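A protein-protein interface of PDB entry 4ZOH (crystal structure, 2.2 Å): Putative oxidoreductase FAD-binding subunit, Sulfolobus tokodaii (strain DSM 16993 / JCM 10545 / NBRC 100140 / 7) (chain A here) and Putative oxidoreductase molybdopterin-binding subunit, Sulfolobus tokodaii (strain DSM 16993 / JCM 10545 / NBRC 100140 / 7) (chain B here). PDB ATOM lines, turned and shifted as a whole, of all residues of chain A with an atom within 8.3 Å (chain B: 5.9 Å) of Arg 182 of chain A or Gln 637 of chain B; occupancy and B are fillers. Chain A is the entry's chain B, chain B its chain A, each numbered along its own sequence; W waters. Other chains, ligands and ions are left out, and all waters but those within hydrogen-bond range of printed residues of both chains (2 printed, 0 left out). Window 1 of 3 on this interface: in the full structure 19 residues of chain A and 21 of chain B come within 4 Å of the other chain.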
ATOM      1  N   ASN A  94      36.883  35.854  -1.963  1.00  0.00           N
ATOM      2  CA  ASN A  94      36.011  34.727  -1.695  1.00  0.00           C
ATOM      3  C   ASN A  94      34.858  34.584  -2.679  1.00  0.00           C
ATOM      4  O   ASN A  94      34.182  33.586  -2.654  1.00  0.00           O
ATOM      5  CB  ASN A  94      35.376  34.900  -0.297  1.00  0.00           C
ATOM      6  CG  ASN A  94      36.322  34.507   0.799  1.00  0.00           C
ATOM      7  OD1 ASN A  94      36.339  33.344   1.210  1.00  0.00           O
ATOM      8  ND2 ASN A  94      37.150  35.459   1.247  1.00  0.00           N
ATOM      9  N   GLY A  96      32.419  33.727  -5.568  1.00  0.00           N
ATOM     10  CA  GLY A  96      32.417  32.716  -6.659  1.00  0.00           C
ATOM     11  C   GLY A  96      33.699  31.977  -7.020  1.00  0.00           C
ATOM     12  O   GLY A  96      34.316  31.328  -6.164  1.00  0.00           O
ATOM     13  N   ASP A 114      21.681  40.063  -3.668  1.00  0.00           N
ATOM     14  CA  ASP A 114      21.428  38.721  -3.186  1.00  0.00           C
ATOM     15  C   ASP A 114      21.735  38.671  -1.673  1.00  0.00           C
ATOM     16  O   ASP A 114      22.819  39.054  -1.266  1.00  0.00           O
ATOM     17  CB  ASP A 114      22.297  37.713  -3.927  1.00  0.00           C
ATOM     18  CG  ASP A 114      21.914  36.310  -3.623  1.00  0.00           C
ATOM     19  OD1 ASP A 114      22.038  35.830  -2.451  1.00  0.00           O
ATOM     20  OD2 ASP A 114      21.467  35.687  -4.576  1.00  0.00           O
ATOM     21  N   LYS A 178      33.815  32.497   5.457  1.00  0.00           N
ATOM     22  CA  LYS A 178      32.765  32.134   4.558  1.00  0.00           C
ATOM     23  C   LYS A 178      32.523  30.664   4.727  1.00  0.00           C
ATOM     24  O   LYS A 178      33.391  29.864   4.457  1.00  0.00           O
ATOM     25  CB  LYS A 178      33.171  32.446   3.119  1.00  0.00           C
ATOM     26  CG  LYS A 178      32.018  32.308   2.139  1.00  0.00           C
ATOM     27  CD  LYS A 178      32.412  32.628   0.711  1.00  0.00           C
ATOM     28  CE  LYS A 178      31.214  32.365  -0.203  1.00  0.00           C
ATOM     29  NZ  LYS A 178      31.336  33.000  -1.529  1.00  0.00           N
ATOM     30  N   LEU A 179      31.326  30.312   5.144  1.00  0.00           N
ATOM     31  CA  LEU A 179      30.976  28.889   5.205  1.00  0.00           C
ATOM     32  C   LEU A 179      30.341  28.486   3.868  1.00  0.00           C
ATOM     33  O   LEU A 179      29.387  29.176   3.370  1.00  0.00           O
ATOM     34  CB  LEU A 179      30.028  28.591   6.391  1.00  0.00           C
ATOM     35  CG  LEU A 179      29.446  27.173   6.532  1.00  0.00           C
ATOM     36  CD1 LEU A 179      30.480  26.088   6.695  1.00  0.00           C
ATOM     37  CD2 LEU A 179      28.473  27.156   7.702  1.00  0.00           C
ATOM     38  N   GLU A 180      30.840  27.371   3.322  1.00  0.00           N
ATOM     39  CA  GLU A 180      30.425  26.878   1.997  1.00  0.00           C
ATOM     40  C   GLU A 180      30.580  25.364   1.882  1.00  0.00           C
ATOM     41  O   GLU A 180      31.543  24.748   2.356  1.00  0.00           O
ATOM     42  CB  GLU A 180      31.211  27.549   0.858  1.00  0.00           C
ATOM     43  CG  GLU A 180      32.719  27.370   0.960  1.00  0.00           C
ATOM     44  CD  GLU A 180      33.508  28.272   0.039  1.00  0.00           C
ATOM     45  OE1 GLU A 180      33.072  29.358  -0.331  1.00  0.00           O
ATOM     46  OE2 GLU A 180      34.602  27.866  -0.327  1.00  0.00           O
ATOM     47  N   ARG A 181      29.633  24.772   1.192  1.00  0.00           N
ATOM     48  CA  ARG A 181      29.726  23.358   0.936  1.00  0.00           C
ATOM     49  C   ARG A 181      30.815  23.048  -0.070  1.00  0.00           C
ATOM     50  O   ARG A 181      31.534  22.059   0.100  1.00  0.00           O
ATOM     51  CB  ARG A 181      28.388  22.860   0.449  1.00  0.00           C
ATOM     52  CG  ARG A 181      28.325  21.342   0.422  1.00  0.00           C
ATOM     53  CD  ARG A 181      26.855  20.925   0.411  1.00  0.00           C
ATOM     54  NE  ARG A 181      26.088  21.686  -0.596  1.00  0.00           N
ATOM     55  CZ  ARG A 181      24.815  21.429  -0.912  1.00  0.00           C
ATOM     56  NH1 ARG A 181      24.130  20.441  -0.278  1.00  0.00           N
ATOM     57  NH2 ARG A 181      24.235  22.163  -1.839  1.00  0.00           N
ATOM     58  N   ARG A 182      30.950  23.892  -1.100  1.00  0.00           N
ATOM     59  CA  ARG A 182      31.949  23.678  -2.136  1.00  0.00           C
ATOM     60  C   ARG A 182      32.552  25.003  -2.514  1.00  0.00           C
ATOM     61  O   ARG A 182      31.858  26.029  -2.494  1.00  0.00           O
ATOM     62  CB  ARG A 182      31.303  23.064  -3.396  1.00  0.00           C
ATOM     63  CG  ARG A 182      30.965  21.578  -3.312  1.00  0.00           C
ATOM     64  CD  ARG A 182      30.342  21.152  -4.639  1.00  0.00           C
ATOM     65  NE  ARG A 182      29.362  22.184  -5.015  1.00  0.00           N
ATOM     66  CZ  ARG A 182      29.065  22.576  -6.246  1.00  0.00           C
ATOM     67  NH1 ARG A 182      29.610  21.949  -7.319  1.00  0.00           N
ATOM     68  NH2 ARG A 182      28.198  23.597  -6.385  1.00  0.00           N
ATOM     69  N   ALA A 183      33.835  24.961  -2.885  1.00  0.00           N
ATOM     70  CA  ALA A 183      34.560  26.152  -3.418  1.00  0.00           C
ATOM     71  C   ALA A 183      33.738  26.634  -4.597  1.00  0.00           C
ATOM     72  O   ALA A 183      33.127  25.804  -5.312  1.00  0.00           O
ATOM     73  CB  ALA A 183      36.001  25.782  -3.823  1.00  0.00           C
ATOM     74  N   GLY A 184      33.578  27.948  -4.706  1.00  0.00           N
ATOM     75  CA  GLY A 184      32.740  28.518  -5.725  1.00  0.00           C
ATOM     76  C   GLY A 184      31.308  28.876  -5.340  1.00  0.00           C
ATOM     77  O   GLY A 184      30.710  29.709  -5.988  1.00  0.00           O
ATOM     78  N   ASP A 185      30.755  28.282  -4.277  1.00  0.00           N
ATOM     79  CA  ASP A 185      29.348  28.521  -3.899  1.00  0.00           C
ATOM     80  C   ASP A 185      29.211  29.910  -3.263  1.00  0.00           C
ATOM     81  O   ASP A 185      30.222  30.465  -2.777  1.00  0.00           O
ATOM     82  CB  ASP A 185      28.889  27.520  -2.823  1.00  0.00           C
ATOM     83  CG  ASP A 185      28.880  26.076  -3.269  1.00  0.00           C
ATOM     84  OD1 ASP A 185      29.035  25.761  -4.476  1.00  0.00           O
ATOM     85  OD2 ASP A 185      28.704  25.212  -2.361  1.00  0.00           O
ATOM     86  N   PHE A 186      27.982  30.447  -3.244  1.00  0.00           N
ATOM     87  CA  PHE A 186      27.581  31.527  -2.377  1.00  0.00           C
ATOM     88  C   PHE A 186      27.706  31.104  -0.882  1.00  0.00           C
ATOM     89  O   PHE A 186      27.720  29.899  -0.521  1.00  0.00           O
ATOM     90  CB  PHE A 186      26.123  31.826  -2.648  1.00  0.00           C
ATOM     91  CG  PHE A 186      25.911  32.774  -3.797  1.00  0.00           C
ATOM     92  CD1 PHE A 186      25.857  34.145  -3.575  1.00  0.00           C
ATOM     93  CD2 PHE A 186      25.804  32.292  -5.142  1.00  0.00           C
ATOM     94  CE1 PHE A 186      25.640  35.034  -4.635  1.00  0.00           C
ATOM     95  CE2 PHE A 186      25.614  33.199  -6.190  1.00  0.00           C
ATOM     96  CZ  PHE A 186      25.522  34.555  -5.932  1.00  0.00           C
ATOM     97  N   ALA A 187      27.796  32.085  -0.010  1.00  0.00           N
ATOM     98  CA  ALA A 187      27.847  31.811   1.449  1.00  0.00           C
ATOM     99  C   ALA A 187      26.618  31.101   2.012  1.00  0.00           C
ATOM    100  O   ALA A 187      25.513  31.525   1.724  1.00  0.00           O
ATOM    101  CB  ALA A 187      28.059  33.113   2.204  1.00  0.00           C
ATOM    102  N   ILE A 188      26.838  30.016   2.767  1.00  0.00           N
ATOM    103  CA  ILE A 188      25.829  29.454   3.667  1.00  0.00           C
ATOM    104  C   ILE A 188      25.722  30.417   4.878  1.00  0.00           C
ATOM    105  O   ILE A 188      24.628  30.782   5.309  1.00  0.00           O
ATOM    106  CB  ILE A 188      26.203  28.044   4.196  1.00  0.00           C
ATOM    107  CG1 ILE A 188      26.114  26.966   3.083  1.00  0.00           C
ATOM    108  CG2 ILE A 188      25.279  27.678   5.372  1.00  0.00           C
ATOM    109  CD1 ILE A 188      26.961  25.752   3.338  1.00  0.00           C
ATOM    110  N   LYS B 582      31.867  20.145   8.468  1.00  0.00           N
ATOM    111  CA  LYS B 582      32.456  19.823   7.182  1.00  0.00           C
ATOM    112  C   LYS B 582      33.488  18.723   7.316  1.00  0.00           C
ATOM    113  O   LYS B 582      34.329  18.749   8.215  1.00  0.00           O
ATOM    114  CB  LYS B 582      33.075  21.083   6.535  1.00  0.00           C
ATOM    115  CG  LYS B 582      33.686  20.792   5.159  1.00  0.00           C
ATOM    116  CD  LYS B 582      34.385  21.980   4.531  1.00  0.00           C
ATOM    117  CE  LYS B 582      33.400  22.965   3.984  1.00  0.00           C
ATOM    118  NZ  LYS B 582      33.846  23.376   2.636  1.00  0.00           N
ATOM    119  N   LEU B 620      28.272  14.586  -0.347  1.00  0.00           N
ATOM    120  CA  LEU B 620      27.770  15.819  -1.012  1.00  0.00           C
ATOM    121  C   LEU B 620      26.422  15.643  -1.664  1.00  0.00           C
ATOM    122  O   LEU B 620      25.539  16.455  -1.446  1.00  0.00           O
ATOM    123  CB  LEU B 620      28.769  16.350  -2.074  1.00  0.00           C
ATOM    124  CG  LEU B 620      30.141  16.911  -1.633  1.00  0.00           C
ATOM    125  CD1 LEU B 620      31.152  16.876  -2.784  1.00  0.00           C
ATOM    126  CD2 LEU B 620      29.939  18.343  -1.177  1.00  0.00           C
ATOM    127  N   ASN B 635      20.426  21.965 -10.752  1.00  0.00           N
ATOM    128  CA  ASN B 635      21.569  22.645 -11.379  1.00  0.00           C
ATOM    129  C   ASN B 635      22.822  22.341 -10.613  1.00  0.00           C
ATOM    130  O   ASN B 635      22.753  21.753  -9.544  1.00  0.00           O
ATOM    131  CB  ASN B 635      21.342  24.134 -11.434  1.00  0.00           C
ATOM    132  CG  ASN B 635      21.053  24.675 -10.089  1.00  0.00           C
ATOM    133  OD1 ASN B 635      21.910  24.640  -9.200  1.00  0.00           O
ATOM    134  ND2 ASN B 635      19.809  25.105  -9.890  1.00  0.00           N
ATOM    135  N   PHE B 636      23.984  22.657 -11.197  1.00  0.00           N
ATOM    136  CA  PHE B 636      25.267  22.342 -10.558  1.00  0.00           C
ATOM    137  C   PHE B 636      25.579  23.163  -9.313  1.00  0.00           C
ATOM    138  O   PHE B 636      26.503  22.810  -8.595  1.00  0.00           O
ATOM    139  CB  PHE B 636      26.441  22.377 -11.532  1.00  0.00           C
ATOM    140  CG  PHE B 636      26.542  21.173 -12.386  1.00  0.00           C
ATOM    141  CD1 PHE B 636      26.606  19.907 -11.821  1.00  0.00           C
ATOM    142  CD2 PHE B 636      26.546  21.307 -13.794  1.00  0.00           C
ATOM    143  CE1 PHE B 636      26.718  18.776 -12.636  1.00  0.00           C
ATOM    144  CE2 PHE B 636      26.685  20.189 -14.601  1.00  0.00           C
ATOM    145  CZ  PHE B 636      26.780  18.909 -14.033  1.00  0.00           C
ATOM    146  N   GLN B 637      24.794  24.197  -9.032  1.00  0.00           N
ATOM    147  CA  GLN B 637      24.873  24.882  -7.718  1.00  0.00           C
ATOM    148  C   GLN B 637      24.168  24.014  -6.707  1.00  0.00           C
ATOM    149  O   GLN B 637      24.820  23.627  -5.771  1.00  0.00           O
ATOM    150  CB  GLN B 637      24.312  26.314  -7.780  1.00  0.00           C
ATOM    151  CG  GLN B 637      24.018  26.994  -6.453  1.00  0.00           C
ATOM    152  CD  GLN B 637      23.130  28.215  -6.658  1.00  0.00           C
ATOM    153  OE1 GLN B 637      23.599  29.304  -6.946  1.00  0.00           O
ATOM    154  NE2 GLN B 637      21.825  28.024  -6.536  1.00  0.00           N
ATOM    155  N   ASP B 638      22.887  23.630  -6.931  1.00  0.00           N
ATOM    156  CA  ASP B 638      22.118  22.866  -5.914  1.00  0.00           C
ATOM    157  C   ASP B 638      22.348  21.343  -5.906  1.00  0.00           C
ATOM    158  O   ASP B 638      22.006  20.666  -4.944  1.00  0.00           O
ATOM    159  CB  ASP B 638      20.597  23.130  -5.994  1.00  0.00           C
ATOM    160  CG  ASP B 638      20.260  24.578  -6.114  1.00  0.00           C
ATOM    161  OD1 ASP B 638      20.926  25.423  -5.486  1.00  0.00           O
ATOM    162  OD2 ASP B 638      19.317  24.894  -6.866  1.00  0.00           O
ATOM    163  N   TYR B 639      22.870  20.780  -6.997  1.00  0.00           N
ATOM    164  CA  TYR B 639      23.309  19.381  -7.001  1.00  0.00           C
ATOM    165  C   TYR B 639      24.844  19.383  -6.992  1.00  0.00           C
ATOM    166  O   TYR B 639      25.465  19.530  -8.033  1.00  0.00           O
ATOM    167  CB  TYR B 639      22.758  18.579  -8.183  1.00  0.00           C
ATOM    168  CG  TYR B 639      23.048  17.113  -7.997  1.00  0.00           C
ATOM    169  CD1 TYR B 639      22.226  16.325  -7.209  1.00  0.00           C
ATOM    170  CD2 TYR B 639      24.165  16.535  -8.581  1.00  0.00           C
ATOM    171  CE1 TYR B 639      22.512  14.966  -7.017  1.00  0.00           C
ATOM    172  CE2 TYR B 639      24.463  15.212  -8.384  1.00  0.00           C
ATOM    173  CZ  TYR B 639      23.631  14.435  -7.568  1.00  0.00           C
ATOM    174  OH  TYR B 639      23.964  13.120  -7.403  1.00  0.00           O
ATOM    175  N   PRO B 640      25.453  19.258  -5.801  1.00  0.00           N
ATOM    176  CA  PRO B 640      26.863  19.689  -5.641  1.00  0.00           C
ATOM    177  C   PRO B 640      27.880  18.637  -6.026  1.00  0.00           C
ATOM    178  O   PRO B 640      28.502  18.016  -5.121  1.00  0.00           O
ATOM    179  CB  PRO B 640      26.942  19.978  -4.126  1.00  0.00           C
ATOM    180  CG  PRO B 640      26.002  18.972  -3.540  1.00  0.00           C
ATOM    181  CD  PRO B 640      24.843  18.877  -4.499  1.00  0.00           C
ATOM    182  N   ILE B 641      28.121  18.424  -7.326  1.00  0.00           N
ATOM    183  CA  ILE B 641      29.197  17.477  -7.645  1.00  0.00           C
ATOM    184  C   ILE B 641      30.544  18.144  -7.177  1.00  0.00           C
ATOM    185  O   ILE B 641      30.630  19.377  -7.162  1.00  0.00           O
ATOM    186  CB  ILE B 641      29.198  17.040  -9.130  1.00  0.00           C
ATOM    187  CG1 ILE B 641      29.664  18.141 -10.109  1.00  0.00           C
ATOM    188  CG2 ILE B 641      27.790  16.556  -9.479  1.00  0.00           C
ATOM    189  CD1 ILE B 641      30.071  17.537 -11.487  1.00  0.00           C
ATOM    190  N   PRO B 642      31.557  17.344  -6.792  1.00  0.00           N
ATOM    191  CA  PRO B 642      32.733  18.027  -6.194  1.00  0.00           C
ATOM    192  C   PRO B 642      33.611  18.822  -7.205  1.00  0.00           C
ATOM    193  O   PRO B 642      33.786  18.401  -8.361  1.00  0.00           O
ATOM    194  CB  PRO B 642      33.565  16.897  -5.606  1.00  0.00           C
ATOM    195  CG  PRO B 642      33.112  15.678  -6.236  1.00  0.00           C
ATOM    196  CD  PRO B 642      31.656  15.875  -6.647  1.00  0.00           C
ATOM    197  N   THR B 643      34.097  19.979  -6.769  1.00  0.00           N
ATOM    198  CA  THR B 643      35.256  20.619  -7.404  1.00  0.00           C
ATOM    199  C   THR B 643      36.575  19.963  -6.966  1.00  0.00           C
ATOM    200  O   THR B 643      36.581  19.065  -6.095  1.00  0.00           O
ATOM    201  CB  THR B 643      35.282  22.111  -7.095  1.00  0.00           C
ATOM    202  OG1 THR B 643      35.816  22.311  -5.766  1.00  0.00           O
ATOM    203  CG2 THR B 643      33.884  22.747  -7.162  1.00  0.00           C
ATOM    204  N   GLU B 646      37.209  19.619  -3.223  1.00  0.00           N
ATOM    205  CA  GLU B 646      36.614  18.620  -2.343  1.00  0.00           C
ATOM    206  C   GLU B 646      37.205  17.201  -2.462  1.00  0.00           C
ATOM    207  O   GLU B 646      36.569  16.273  -2.091  1.00  0.00           O
ATOM    208  CB  GLU B 646      35.086  18.626  -2.482  1.00  0.00           C
ATOM    209  CG  GLU B 646      34.445  19.875  -1.903  1.00  0.00           C
ATOM    210  CD  GLU B 646      34.565  21.079  -2.835  1.00  0.00           C
ATOM    211  OE1 GLU B 646      34.408  20.903  -4.084  1.00  0.00           O
ATOM    212  OE2 GLU B 646      34.832  22.193  -2.333  1.00  0.00           O
HETATM  213  O   HOH W   1      25.137  18.028   0.665  1.00  0.00           O
HETATM  214  O   HOH W   2      21.771  21.466  -2.429  1.00  0.00           O
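NZ of Lys 582 of chain B touches O of Arg 181 of chain A, 3.7 Å away. Leu 620 of chain B touches Arg 181 of chain A (CD2 to CG, 3.8 Å). Arg 181 of chain A touches Pro 640 of chain B (CZ to CG, 3.8 Å). Pro 640 of chain B touches Arg 182 of chain A (CB to NE, 3.4 Å). CA of Arg 182 of chain A touches OE2 of Glu 646 of chain B, at 3.2 Å. O of Ala 183 of chain A touches CG2 of Thr 643 of chain B, at 3.7 Å.
Water W2 bridges NH2 of Arg 181 of chain A (2.6 Å) and O of Asp 638 of chain B (2.6 Å). Water W1 lies within hydrogen-bond range of the backbone carbonyl oxygen (O) of Leu 620 of chain B and the guanidinium group (NH1) of Arg 181 of chain A.
Of the 12 printed residues of chain B, 8 touch a printed residue of chain A. Hydrophobic or aromatic side chains of chain A within 4 Å of the printed part of chain B: Ala 183. Among the printed residues, 11 pairs touch across the chains.
The backbone NH (N) of Ala 183 of chain A sits at hydrogen-bond distance from the side-chain carboxylate (OE2) of Glu 646 of chain B (3.0 Å). The side-chain amino group (NZ) of Lys 582 of chain B sits at hydrogen-bond distance from the backbone carbonyl oxygen (O) of Glu 180 of chain A, 2.7 Å away. O of Ile 641 of chain B is in hydrogen-bond range of NH1 of Arg 182 of chain A (2.8 Å). The backbone carbonyl oxygen of Gln 637 of chain B lies within hydrogen-bond range of the guanidinium group of Arg 182 of chain A. The guanidinium group (NH2) of Arg 182 of chain A sits at hydrogen-bond distance from the backbone carbonyl oxygen (O) of Phe 636 of chain B (2.9 Å).
The side-chain hydroxyl (OG1) of Thr 643 of chain B sits at hydrogen-bond distance from the side-chain carboxylate (OE1) of Glu 646 of chain B, at 2.6 Å. The side-chain amide nitrogen of Gln 637 of chain B lies within hydrogen-bond range of the side-chain carboxylate of Asp 638 of chain B. NH2 of Arg 182 of chain A is in salt-bridge range of OD1 of Asp 185 of chain A (3.0 Å). The backbone NH (N) of Gln 637 of chain B sits at hydrogen-bond distance from the side-chain amide oxygen (OD1) of Asn 635 of chain B, at 2.9 Å.
Printed residues of chain B within 4 Å of Arg 182 of chain A: Phe 636 (2.9 Å), Gln 637 (3.4 Å), Pro 640 (3.4 Å), Ile 641 (2.8 Å) and Glu 646 (3.2 Å). Gln 637 of chain B touches one residue of chain A. No residue of chain A comes within 4 Å of Asp 638 of chain B. Printed residues of chain A within 4 Å of Pro 640 of chain B: Arg 181 (3.8 Å) and Arg 182 (3.4 Å). Of the printed residues of chain B, Ala 183 of chain A touches Thr 643 (3.7 Å) and Glu 646 (3.0 Å). The nearest printed residue of chain B that does not touch Arg 182 of chain A is Leu 620 of chain B (4.01 Å). The nearest residue of chain A that does not touch Gln 637 of chain B is Phe 186 of chain A (4.1 Å).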
